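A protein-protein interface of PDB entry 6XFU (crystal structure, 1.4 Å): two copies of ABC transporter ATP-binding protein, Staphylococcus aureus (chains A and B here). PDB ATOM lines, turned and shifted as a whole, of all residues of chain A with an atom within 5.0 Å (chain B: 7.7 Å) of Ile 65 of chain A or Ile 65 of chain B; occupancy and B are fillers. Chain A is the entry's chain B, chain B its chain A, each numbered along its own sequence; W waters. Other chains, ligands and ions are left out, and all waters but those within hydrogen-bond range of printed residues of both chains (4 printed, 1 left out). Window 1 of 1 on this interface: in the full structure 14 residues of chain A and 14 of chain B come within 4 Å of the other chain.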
ATOM      1  N   THR A   8      10.593  17.551   5.748  1.00  0.00           N
ATOM      2  CA  THR A   8      12.000  17.445   5.302  1.00  0.00           C
ATOM      3  C   THR A   8      12.034  16.329   4.259  1.00  0.00           C
ATOM      4  O   THR A   8      11.531  15.220   4.559  1.00  0.00           O
ATOM      5  CB  THR A   8      12.998  17.221   6.408  1.00  0.00           C
ATOM      6  OG1 THR A   8      13.000  18.433   7.190  1.00  0.00           O
ATOM      7  CG2 THR A   8      14.397  16.949   5.910  1.00  0.00           C
ATOM      8  N   ILE A   9      12.547  16.625   3.100  1.00  0.00           N
ATOM      9  CA  ILE A   9      12.658  15.667   1.965  1.00  0.00           C
ATOM     10  C   ILE A   9      14.113  15.263   1.839  1.00  0.00           C
ATOM     11  O   ILE A   9      14.966  16.128   1.655  1.00  0.00           O
ATOM     12  CB  ILE A   9      12.155  16.205   0.630  1.00  0.00           C
ATOM     13  CG1 ILE A   9      10.746  16.782   0.726  1.00  0.00           C
ATOM     14  CG2 ILE A   9      12.214  15.071  -0.398  1.00  0.00           C
ATOM     15  CD1 ILE A   9      10.706  18.245   1.025  1.00  0.00           C
ATOM     16  N   VAL A  10      14.370  13.984   1.947  1.00  0.00           N
ATOM     17  CA  VAL A  10      15.714  13.401   1.787  1.00  0.00           C
ATOM     18  C   VAL A  10      15.701  12.696   0.453  1.00  0.00           C
ATOM     19  O   VAL A  10      14.803  11.867   0.229  1.00  0.00           O
ATOM     20  CB  VAL A  10      16.071  12.480   2.940  1.00  0.00           C
ATOM     21  CG1 VAL A  10      17.470  11.911   2.742  1.00  0.00           C
ATOM     22  CG2 VAL A  10      15.942  13.145   4.300  1.00  0.00           C
ATOM     23  N   THR A  11      16.650  12.979  -0.402  1.00  0.00           N
ATOM     24  CA  THR A  11      16.726  12.374  -1.743  1.00  0.00           C
ATOM     25  C   THR A  11      17.985  11.545  -1.797  1.00  0.00           C
ATOM     26  O   THR A  11      19.071  12.048  -1.481  1.00  0.00           O
ATOM     27  CB  THR A  11      16.691  13.413  -2.848  1.00  0.00           C
ATOM     28  OG1 THR A  11      15.524  14.250  -2.690  1.00  0.00           O
ATOM     29  CG2 THR A  11      16.706  12.796  -4.225  1.00  0.00           C
ATOM     30  N   TYR A  48      19.832  19.066  10.618  1.00  0.00           N
ATOM     31  CA  TYR A  48      20.062  17.851   9.829  1.00  0.00           C
ATOM     32  C   TYR A  48      21.181  16.975  10.378  1.00  0.00           C
ATOM     33  O   TYR A  48      21.373  15.906   9.789  1.00  0.00           O
ATOM     34  CB  TYR A  48      20.392  18.236   8.399  1.00  0.00           C
ATOM     35  CG  TYR A  48      19.336  18.995   7.640  1.00  0.00           C
ATOM     36  CD1 TYR A  48      18.001  18.980   7.993  1.00  0.00           C
ATOM     37  CD2 TYR A  48      19.660  19.628   6.462  1.00  0.00           C
ATOM     38  CE1 TYR A  48      17.040  19.650   7.264  1.00  0.00           C
ATOM     39  CE2 TYR A  48      18.709  20.268   5.688  1.00  0.00           C
ATOM     40  CZ  TYR A  48      17.379  20.261   6.075  1.00  0.00           C
ATOM     41  OH  TYR A  48      16.460  20.863   5.261  1.00  0.00           O
ATOM     42  N   ILE A  51      20.450  13.060  11.349  1.00  0.00           N
ATOM     43  CA  ILE A  51      20.080  12.235  10.191  1.00  0.00           C
ATOM     44  C   ILE A  51      21.303  12.056   9.322  1.00  0.00           C
ATOM     45  O   ILE A  51      21.544  10.920   8.855  1.00  0.00           O
ATOM     46  CB  ILE A  51      18.952  12.842   9.387  1.00  0.00           C
ATOM     47  CG1 ILE A  51      17.664  12.690  10.185  1.00  0.00           C
ATOM     48  CG2 ILE A  51      18.855  12.237   8.003  1.00  0.00           C
ATOM     49  CD1 ILE A  51      16.520  13.439   9.582  1.00  0.00           C
ATOM     50  N   LEU A  52      22.058  13.128   9.060  1.00  0.00           N
ATOM     51  CA  LEU A  52      23.198  12.952   8.130  1.00  0.00           C
ATOM     52  C   LEU A  52      24.258  12.032   8.770  1.00  0.00           C
ATOM     53  O   LEU A  52      24.809  11.210   8.004  1.00  0.00           O
ATOM     54  CB  LEU A  52      23.772  14.320   7.753  1.00  0.00           C
ATOM     55  CG  LEU A  52      22.853  15.198   6.917  1.00  0.00           C
ATOM     56  CD1 LEU A  52      23.468  16.568   6.726  1.00  0.00           C
ATOM     57  CD2 LEU A  52      22.537  14.552   5.570  1.00  0.00           C
ATOM     58  N   LYS A  63      21.777  12.674  -2.072  1.00  0.00           N
ATOM     59  CA  LYS A  63      21.859  13.579  -3.225  1.00  0.00           C
ATOM     60  C   LYS A  63      21.312  14.972  -2.883  1.00  0.00           C
ATOM     61  O   LYS A  63      21.738  15.952  -3.459  1.00  0.00           O
ATOM     62  CB  LYS A  63      21.099  13.056  -4.432  1.00  0.00           C
ATOM     63  CG  LYS A  63      21.527  11.683  -4.910  1.00  0.00           C
ATOM     64  CD  LYS A  63      20.534  11.103  -5.879  1.00  0.00           C
ATOM     65  CE  LYS A  63      20.179  12.007  -7.027  1.00  0.00           C
ATOM     66  NZ  LYS A  63      19.317  11.285  -8.013  1.00  0.00           N
ATOM     67  N   TYR A  64      20.324  15.036  -2.011  1.00  0.00           N
ATOM     68  CA  TYR A  64      19.693  16.332  -1.706  1.00  0.00           C
ATOM     69  C   TYR A  64      18.985  16.190  -0.374  1.00  0.00           C
ATOM     70  O   TYR A  64      18.572  15.087   0.029  1.00  0.00           O
ATOM     71  CB  TYR A  64      18.687  16.762  -2.775  1.00  0.00           C
ATOM     72  CG  TYR A  64      18.650  18.251  -3.013  1.00  0.00           C
ATOM     73  CD1 TYR A  64      19.707  18.872  -3.672  1.00  0.00           C
ATOM     74  CD2 TYR A  64      17.591  19.045  -2.591  1.00  0.00           C
ATOM     75  CE1 TYR A  64      19.707  20.229  -3.945  1.00  0.00           C
ATOM     76  CE2 TYR A  64      17.586  20.414  -2.868  1.00  0.00           C
ATOM     77  CZ  TYR A  64      18.640  20.991  -3.543  1.00  0.00           C
ATOM     78  OH  TYR A  64      18.586  22.341  -3.807  1.00  0.00           O
ATOM     79  N   ILE A  65      18.812  17.302   0.303  1.00  0.00           N
ATOM     80  CA  ILE A  65      17.949  17.412   1.506  1.00  0.00           C
ATOM     81  C   ILE A  65      17.390  18.814   1.512  1.00  0.00           C
ATOM     82  O   ILE A  65      18.133  19.750   1.218  1.00  0.00           O
ATOM     83  CB  ILE A  65      18.700  16.990   2.781  1.00  0.00           C
ATOM     84  CG1 ILE A  65      17.813  16.970   4.039  1.00  0.00           C
ATOM     85  CG2 ILE A  65      19.942  17.834   3.003  1.00  0.00           C
ATOM     86  CD1 ILE A  65      18.415  16.218   5.154  1.00  0.00           C
ATOM     87  N   GLU A  66      16.099  18.929   1.773  1.00  0.00           N
ATOM     88  CA  GLU A  66      15.471  20.265   1.813  1.00  0.00           C
ATOM     89  C   GLU A  66      14.245  20.215   2.710  1.00  0.00           C
ATOM     90  O   GLU A  66      13.757  19.123   2.983  1.00  0.00           O
ATOM     91  CB  GLU A  66      15.156  20.787   0.411  1.00  0.00           C
ATOM     92  CG  GLU A  66      13.949  20.161  -0.244  1.00  0.00           C
ATOM     93  CD  GLU A  66      13.570  20.892  -1.518  1.00  0.00           C
ATOM     94  OE1 GLU A  66      12.960  21.964  -1.420  1.00  0.00           O
ATOM     95  OE2 GLU A  66      13.896  20.396  -2.602  1.00  0.00           O
ATOM     96  N   THR A  67      13.830  21.371   3.196  1.00  0.00           N
ATOM     97  CA  THR A  67      12.602  21.451   4.007  1.00  0.00           C
ATOM     98  C   THR A  67      11.632  22.374   3.299  1.00  0.00           C
ATOM     99  O   THR A  67      12.051  23.446   2.866  1.00  0.00           O
ATOM    100  CB  THR A  67      12.948  21.847   5.431  1.00  0.00           C
ATOM    101  OG1 THR A  67      13.797  20.864   6.039  1.00  0.00           O
ATOM    102  CG2 THR A  67      11.702  22.003   6.287  1.00  0.00           C
ATOM    103  N   THR B   8      24.457  27.874  -2.750  1.00  0.00           N
ATOM    104  CA  THR B   8      24.291  26.800  -1.742  1.00  0.00           C
ATOM    105  C   THR B   8      24.931  27.319  -0.450  1.00  0.00           C
ATOM    106  O   THR B   8      26.105  27.735  -0.466  1.00  0.00           O
ATOM    107  CB  THR B   8      24.872  25.475  -2.187  1.00  0.00           C
ATOM    108  OG1 THR B   8      24.093  24.976  -3.279  1.00  0.00           O
ATOM    109  CG2 THR B   8      24.886  24.446  -1.085  1.00  0.00           C
ATOM    110  N   ILE B   9      24.182  27.270   0.627  1.00  0.00           N
ATOM    111  CA  ILE B   9      24.577  27.741   1.974  1.00  0.00           C
ATOM    112  C   ILE B   9      24.739  26.520   2.855  1.00  0.00           C
ATOM    113  O   ILE B   9      23.772  25.782   3.047  1.00  0.00           O
ATOM    114  CB  ILE B   9      23.568  28.713   2.581  1.00  0.00           C
ATOM    115  CG1 ILE B   9      23.188  29.844   1.639  1.00  0.00           C
ATOM    116  CG2 ILE B   9      24.145  29.248   3.898  1.00  0.00           C
ATOM    117  CD1 ILE B   9      21.873  30.481   2.054  1.00  0.00           C
ATOM    118  N   VAL B  10      25.921  26.320   3.381  1.00  0.00           N
ATOM    119  CA  VAL B  10      26.217  25.236   4.346  1.00  0.00           C
ATOM    120  C   VAL B  10      26.281  25.879   5.716  1.00  0.00           C
ATOM    121  O   VAL B  10      27.026  26.862   5.903  1.00  0.00           O
ATOM    122  CB  VAL B  10      27.524  24.551   3.964  1.00  0.00           C
ATOM    123  CG1 VAL B  10      27.873  23.430   4.935  1.00  0.00           C
ATOM    124  CG2 VAL B  10      27.456  23.977   2.564  1.00  0.00           C
ATOM    125  N   THR B  11      25.621  25.314   6.685  1.00  0.00           N
ATOM    126  CA  THR B  11      25.634  25.785   8.081  1.00  0.00           C
ATOM    127  C   THR B  11      26.191  24.656   8.955  1.00  0.00           C
ATOM    128  O   THR B  11      25.687  23.533   8.926  1.00  0.00           O
ATOM    129  CB  THR B  11      24.265  26.214   8.560  1.00  0.00           C
ATOM    130  OG1 THR B  11      23.794  27.223   7.643  1.00  0.00           O
ATOM    131  CG2 THR B  11      24.295  26.767   9.966  1.00  0.00           C
ATOM    132  N   VAL B  12      27.230  24.994   9.715  1.00  0.00           N
ATOM    133  CA  VAL B  12      27.898  24.029  10.623  1.00  0.00           C
ATOM    134  C   VAL B  12      27.977  24.613  12.026  1.00  0.00           C
ATOM    135  O   VAL B  12      27.879  25.839  12.233  1.00  0.00           O
ATOM    136  CB  VAL B  12      29.280  23.644  10.086  1.00  0.00           C
ATOM    137  CG1 VAL B  12      29.194  22.847   8.793  1.00  0.00           C
ATOM    138  CG2 VAL B  12      30.187  24.845   9.941  1.00  0.00           C
ATOM    139  N   LEU B  40      28.592  29.257   5.304  1.00  0.00           N
ATOM    140  CA  LEU B  40      29.543  29.242   4.159  1.00  0.00           C
ATOM    141  C   LEU B  40      28.690  29.212   2.899  1.00  0.00           C
ATOM    142  O   LEU B  40      27.764  28.390   2.850  1.00  0.00           O
ATOM    143  CB  LEU B  40      30.401  27.974   4.094  1.00  0.00           C
ATOM    144  CG  LEU B  40      31.357  27.607   5.221  1.00  0.00           C
ATOM    145  CD1 LEU B  40      32.418  28.636   5.487  1.00  0.00           C
ATOM    146  CD2 LEU B  40      30.680  27.078   6.464  1.00  0.00           C
ATOM    147  N   ILE B  42      28.692  28.827  -1.344  1.00  0.00           N
ATOM    148  CA  ILE B  42      29.385  28.407  -2.586  1.00  0.00           C
ATOM    149  C   ILE B  42      28.428  28.564  -3.760  1.00  0.00           C
ATOM    150  O   ILE B  42      27.215  28.739  -3.577  1.00  0.00           O
ATOM    151  CB  ILE B  42      29.957  26.986  -2.461  1.00  0.00           C
ATOM    152  CG1 ILE B  42      28.833  25.987  -2.223  1.00  0.00           C
ATOM    153  CG2 ILE B  42      31.047  26.924  -1.396  1.00  0.00           C
ATOM    154  CD1 ILE B  42      29.275  24.534  -2.295  1.00  0.00           C
ATOM    155  N   GLN B  45      24.875  24.003  -5.892  1.00  0.00           N
ATOM    156  CA  GLN B  45      25.125  22.605  -6.214  1.00  0.00           C
ATOM    157  C   GLN B  45      23.796  21.892  -6.412  1.00  0.00           C
ATOM    158  O   GLN B  45      22.900  22.015  -5.582  1.00  0.00           O
ATOM    159  CB  GLN B  45      25.935  21.942  -5.107  1.00  0.00           C
ATOM    160  CG  GLN B  45      27.257  22.650  -4.870  1.00  0.00           C
ATOM    161  CD  GLN B  45      28.194  22.614  -6.050  1.00  0.00           C
ATOM    162  OE1 GLN B  45      28.445  21.553  -6.649  1.00  0.00           O
ATOM    163  NE2 GLN B  45      28.753  23.771  -6.389  1.00  0.00           N
ATOM    164  N   LYS B  46      23.662  21.121  -7.478  1.00  0.00           N
ATOM    165  CA  LYS B  46      22.417  20.347  -7.700  1.00  0.00           C
ATOM    166  C   LYS B  46      22.412  19.027  -6.933  1.00  0.00           C
ATOM    167  O   LYS B  46      21.343  18.444  -6.719  1.00  0.00           O
ATOM    168  CB  LYS B  46      22.277  20.021  -9.187  1.00  0.00           C
ATOM    169  CG  LYS B  46      22.231  21.216 -10.119  1.00  0.00           C
ATOM    170  CD  LYS B  46      21.070  22.110  -9.903  1.00  0.00           C
ATOM    171  CE  LYS B  46      20.652  22.834 -11.177  1.00  0.00           C
ATOM    172  NZ  LYS B  46      21.723  23.719 -11.679  1.00  0.00           N
ATOM    173  N   ASN B  47      23.569  18.514  -6.574  1.00  0.00           N
ATOM    174  CA  ASN B  47      23.734  17.198  -5.947  1.00  0.00           C
ATOM    175  C   ASN B  47      24.735  17.364  -4.801  1.00  0.00           C
ATOM    176  O   ASN B  47      25.871  17.811  -5.021  1.00  0.00           O
ATOM    177  CB  ASN B  47      24.155  16.162  -6.988  1.00  0.00           C
ATOM    178  CG  ASN B  47      24.308  14.757  -6.441  1.00  0.00           C
ATOM    179  OD1 ASN B  47      24.710  14.534  -5.323  1.00  0.00           O
ATOM    180  ND2 ASN B  47      23.970  13.734  -7.225  1.00  0.00           N
ATOM    181  N   TYR B  48      24.295  17.108  -3.582  1.00  0.00           N
ATOM    182  CA  TYR B  48      25.080  17.359  -2.354  1.00  0.00           C
ATOM    183  C   TYR B  48      25.993  16.211  -1.966  1.00  0.00           C
ATOM    184  O   TYR B  48      26.722  16.292  -0.990  1.00  0.00           O
ATOM    185  CB  TYR B  48      24.134  17.620  -1.184  1.00  0.00           C
ATOM    186  CG  TYR B  48      23.229  18.819  -1.284  1.00  0.00           C
ATOM    187  CD1 TYR B  48      23.478  19.882  -2.142  1.00  0.00           C
ATOM    188  CD2 TYR B  48      22.160  18.960  -0.408  1.00  0.00           C
ATOM    189  CE1 TYR B  48      22.708  21.035  -2.152  1.00  0.00           C
ATOM    190  CE2 TYR B  48      21.393  20.108  -0.392  1.00  0.00           C
ATOM    191  CZ  TYR B  48      21.663  21.157  -1.253  1.00  0.00           C
ATOM    192  OH  TYR B  48      20.879  22.285  -1.269  1.00  0.00           O
ATOM    193  N   GLN B  49      25.973  15.119  -2.709  1.00  0.00           N
ATOM    194  CA  GLN B  49      26.635  13.870  -2.248  1.00  0.00           C
ATOM    195  C   GLN B  49      28.146  14.076  -2.100  1.00  0.00           C
ATOM    196  O   GLN B  49      28.705  13.606  -1.124  1.00  0.00           O
ATOM    197  CB  GLN B  49      26.337  12.732  -3.234  1.00  0.00           C
ATOM    198  CG  GLN B  49      26.734  11.350  -2.751  1.00  0.00           C
ATOM    199  CD  GLN B  49      26.145  10.332  -3.700  1.00  0.00           C
ATOM    200  OE1 GLN B  49      26.439  10.353  -4.893  1.00  0.00           O
ATOM    201  NE2 GLN B  49      25.140   9.605  -3.227  1.00  0.00           N
ATOM    202  N   ILE B  51      29.895  16.770  -1.393  1.00  0.00           N
ATOM    203  CA  ILE B  51      30.194  17.584  -0.192  1.00  0.00           C
ATOM    204  C   ILE B  51      29.866  16.798   1.048  1.00  0.00           C
ATOM    205  O   ILE B  51      30.657  16.788   2.000  1.00  0.00           O
ATOM    206  CB  ILE B  51      29.416  18.902  -0.250  1.00  0.00           C
ATOM    207  CG1 ILE B  51      30.026  19.836  -1.281  1.00  0.00           C
ATOM    208  CG2 ILE B  51      29.366  19.571   1.108  1.00  0.00           C
ATOM    209  CD1 ILE B  51      29.128  20.962  -1.690  1.00  0.00           C
ATOM    210  N   LEU B  52      28.686  16.167   1.103  1.00  0.00           N
ATOM    211  CA  LEU B  52      28.306  15.464   2.340  1.00  0.00           C
ATOM    212  C   LEU B  52      29.291  14.330   2.608  1.00  0.00           C
ATOM    213  O   LEU B  52      29.649  14.130   3.755  1.00  0.00           O
ATOM    214  CB  LEU B  52      26.862  15.006   2.261  1.00  0.00           C
ATOM    215  CG  LEU B  52      25.857  16.149   2.229  1.00  0.00           C
ATOM    216  CD1 LEU B  52      24.446  15.589   2.051  1.00  0.00           C
ATOM    217  CD2 LEU B  52      25.978  17.016   3.486  1.00  0.00           C
ATOM    218  N   LEU B  55      32.671  15.866   3.857  1.00  0.00           N
ATOM    219  CA  LEU B  55      32.540  16.390   5.234  1.00  0.00           C
ATOM    220  C   LEU B  55      32.440  15.217   6.218  1.00  0.00           C
ATOM    221  O   LEU B  55      32.992  15.311   7.296  1.00  0.00           O
ATOM    222  CB  LEU B  55      31.361  17.357   5.315  1.00  0.00           C
ATOM    223  CG  LEU B  55      31.579  18.708   4.608  1.00  0.00           C
ATOM    224  CD1 LEU B  55      30.324  19.540   4.738  1.00  0.00           C
ATOM    225  CD2 LEU B  55      32.759  19.481   5.122  1.00  0.00           C
ATOM    226  N   PRO B  62      26.722  18.864   8.581  1.00  0.00           N
ATOM    227  CA  PRO B  62      26.080  20.162   8.654  1.00  0.00           C
ATOM    228  C   PRO B  62      24.815  20.147   9.505  1.00  0.00           C
ATOM    229  O   PRO B  62      24.013  19.213   9.461  1.00  0.00           O
ATOM    230  CB  PRO B  62      25.758  20.466   7.223  1.00  0.00           C
ATOM    231  CG  PRO B  62      26.755  19.683   6.404  1.00  0.00           C
ATOM    232  CD  PRO B  62      26.935  18.404   7.197  1.00  0.00           C
ATOM    233  N   LYS B  63      24.579  21.250  10.209  1.00  0.00           N
ATOM    234  CA  LYS B  63      23.265  21.541  10.803  1.00  0.00           C
ATOM    235  C   LYS B  63      22.239  21.839   9.731  1.00  0.00           C
ATOM    236  O   LYS B  63      21.044  21.533   9.910  1.00  0.00           O
ATOM    237  CB  LYS B  63      23.356  22.809  11.654  1.00  0.00           C
ATOM    238  CG  LYS B  63      24.323  22.687  12.816  1.00  0.00           C
ATOM    239  CD  LYS B  63      24.530  23.972  13.618  1.00  0.00           C
ATOM    240  CE  LYS B  63      23.277  24.426  14.333  1.00  0.00           C
ATOM    241  NZ  LYS B  63      23.529  25.697  15.062  1.00  0.00           N
ATOM    242  N   TYR B  64      22.644  22.400   8.610  1.00  0.00           N
ATOM    243  CA  TYR B  64      21.715  22.745   7.556  1.00  0.00           C
ATOM    244  C   TYR B  64      22.470  22.877   6.260  1.00  0.00           C
ATOM    245  O   TYR B  64      23.659  23.194   6.257  1.00  0.00           O
ATOM    246  CB  TYR B  64      20.986  24.046   7.859  1.00  0.00           C
ATOM    247  CG  TYR B  64      19.543  24.033   7.470  1.00  0.00           C
ATOM    248  CD1 TYR B  64      18.631  23.241   8.146  1.00  0.00           C
ATOM    249  CD2 TYR B  64      19.096  24.762   6.380  1.00  0.00           C
ATOM    250  CE1 TYR B  64      17.296  23.264   7.811  1.00  0.00           C
ATOM    251  CE2 TYR B  64      17.750  24.779   6.013  1.00  0.00           C
ATOM    252  CZ  TYR B  64      16.873  24.003   6.733  1.00  0.00           C
ATOM    253  OH  TYR B  64      15.521  23.972   6.445  1.00  0.00           O
ATOM    254  N   ILE B  65      21.773  22.683   5.156  1.00  0.00           N
ATOM    255  CA  ILE B  65      22.295  22.930   3.815  1.00  0.00           C
ATOM    256  C   ILE B  65      21.076  23.355   3.022  1.00  0.00           C
ATOM    257  O   ILE B  65      20.028  22.738   3.175  1.00  0.00           O
ATOM    258  CB  ILE B  65      23.098  21.761   3.227  1.00  0.00           C
ATOM    259  CG1 ILE B  65      23.665  22.146   1.852  1.00  0.00           C
ATOM    260  CG2 ILE B  65      22.291  20.478   3.198  1.00  0.00           C
ATOM    261  CD1 ILE B  65      24.750  21.194   1.394  1.00  0.00           C
ATOM    262  N   GLU B  66      21.193  24.413   2.229  1.00  0.00           N
ATOM    263  CA  GLU B  66      20.046  25.033   1.520  1.00  0.00           C
ATOM    264  C   GLU B  66      20.575  25.598   0.219  1.00  0.00           C
ATOM    265  O   GLU B  66      21.714  26.102   0.177  1.00  0.00           O
ATOM    266  CB  GLU B  66      19.422  26.117   2.403  1.00  0.00           C
ATOM    267  CG  GLU B  66      18.227  26.847   1.826  1.00  0.00           C
ATOM    268  CD  GLU B  66      17.682  27.965   2.683  1.00  0.00           C
ATOM    269  OE1 GLU B  66      18.281  28.289   3.772  1.00  0.00           O
ATOM    270  OE2 GLU B  66      16.641  28.513   2.260  1.00  0.00           O
ATOM    271  N   THR B  67      19.800  25.488  -0.841  1.00  0.00           N
ATOM    272  CA  THR B  67      20.091  26.177  -2.112  1.00  0.00           C
ATOM    273  C   THR B  67      18.940  27.119  -2.400  1.00  0.00           C
ATOM    274  O   THR B  67      17.789  26.679  -2.323  1.00  0.00           O
ATOM    275  CB  THR B  67      20.373  25.187  -3.243  1.00  0.00           C
ATOM    276  OG1 THR B  67      21.471  24.345  -2.869  1.00  0.00           O
ATOM    277  CG2 THR B  67      20.742  25.882  -4.530  1.00  0.00           C
HETATM  278  O   HOH W   1      16.433  23.778  -3.255  1.00  0.00           O
HETATM  279  O   HOH W   2      14.039  22.679   8.570  1.00  0.00           O
HETATM  280  O   HOH W   3      20.275  22.857  -6.046  1.00  0.00           O
HETATM  281  O   HOH W   4      18.687  22.127   0.236  1.00  0.00           O
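Thr 8 of chain A touches none of the printed residues of chain B. Of the printed residues of chain B, Tyr 48 of chain A touches Pro 62, Lys 63, Tyr 64 and Ile 65. Of chain B, only Tyr 48 (3.7 Å) and Ile 65 (3.5 Å) come within 4 Å of Ile 65 of chain A. Of the printed residues of chain B, Thr 67 of chain A touches Tyr 64 (3.5 Å). Of the printed residues of chain A, Tyr 48 of chain B touches Lys 63, Tyr 64 and Ile 65. Leu 52 of chain B touches none of the printed residues of chain A. Of the printed residues of chain A, Tyr 64 of chain B touches Tyr 48 and Thr 67. Of chain A, only Tyr 48 (3.8 Å) and Ile 65 (3.5 Å) come within 4 Å of Ile 65 of chain B. Of the printed residues of chain A, Thr 67 of chain B touches Tyr 64. The nearest printed residue of chain B that does not touch Lys 63 of chain A is Lys 46 of chain B (4.1 Å).
Among the printed residues, no Asp or Glu carboxylate lies within 4 Å of a Lys or Arg side-chain nitrogen of the other chain.
Water W4 lies within hydrogen-bond range of the backbone carbonyl oxygen (O) of Ile 65 of chain A (2.6 Å), the side-chain hydroxyl (OH) of Tyr 48 of chain B (2.7 Å) and the backbone carbonyl oxygen (O) of Ile 65 of chain B (3.3 Å). Water W1 lies within hydrogen-bond range of OH of Tyr 64 of chain A (2.6 Å) and O of Thr 67 of chain B (3.3 Å). Water W3 bridges the backbone carbonyl oxygen of Gln 45 of chain B (2.8 Å) and the side-chain hydroxyl of Tyr 64 of chain A (2.9 Å). Water W2 bridges the side-chain hydroxyl (OH) of Tyr 64 of chain B (2.9 Å) and the side-chain hydroxyl (OG1) of Thr 67 of chain A (3.1 Å).
Among the printed residues, pairs that only touch across the chains: Tyr 48 of chain A with Pro 62 of chain B (3.7 Å), Tyr 48 of chain A with Ile 65 of chain B (3.8 Å), Leu 52 of chain A with Pro 62 of chain B (3.8 Å), Lys 63 of chain A with Asn 47 of chain B (3.4 Å), Tyr 64 of chain A with Lys 46 of chain B (3.5 Å), Tyr 64 of chain A with Thr 67 of chain B (3.4 Å), Ile 65 of chain A with Tyr 48 of chain B (3.7 Å), Ile 65 of chain A with Ile 65 of chain B (3.5 Å) and Thr 67 of chain A with Tyr 64 of chain B (3.5 Å).
O of Lys 63 of chain B lies within hydrogen-bond range of N of Tyr 48 of chain A, at 2.8 Å. The backbone NH (N) of Tyr 48 of chain B lies within hydrogen-bond range of the backbone carbonyl oxygen (O) of Lys 63 of chain A (2.8 Å). OH of Tyr 48 of chain B is in hydrogen-bond range of OH of Tyr 64 of chain A (3.4 Å). The side-chain hydroxyl (OH) of Tyr 48 of chain A is in hydrogen-bond range of the side-chain hydroxyl (OH) of Tyr 64 of chain B (3.5 Å).
Tyr 48 of chain A touches Lys 63 of chain B, and with the chains exchanged Lys 63 of chain A touches Tyr 48 of chain B. Tyr 48 of chain A touches Tyr 64 of chain B, and with the chains exchanged Tyr 64 of chain A touches Tyr 48 of chain B. Tyr 48 of chain A touches Ile 65 of chain B, and with the chains exchanged Ile 65 of chain A touches Tyr 48 of chain B. Tyr 64 of chain A touches Thr 67 of chain B, and with the chains exchanged Thr 67 of chain A touches Tyr 64 of chain B. 12 positions are printed for both chains.
The backbone carbonyl oxygen (O) of Thr 11 of chain B sits at hydrogen-bond distance from the backbone NH (N) of Lys 63 of chain B (2.8 Å). The backbone NH (N) of Gln 49 of chain B sits at hydrogen-bond distance from the side-chain amide oxygen (OD1) of Asn 47 of chain B (3.0 Å). N of Thr 11 of chain B is in hydrogen-bond range of O of Tyr 64 of chain B (2.9 Å). OH of Tyr 48 of chain A lies within hydrogen-bond range of OG1 of Thr 67 of chain A (2.8 Å). The side-chain hydroxyl of Thr 67 of chain B sits at hydrogen-bond distance from the side-chain hydroxyl of Tyr 48 of chain B (2.7 Å). The side-chain hydroxyl (OG1) of Thr 8 of chain B lies within hydrogen-bond range of the side-chain hydroxyl (OG1) of Thr 67 of chain B (2.7 Å).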
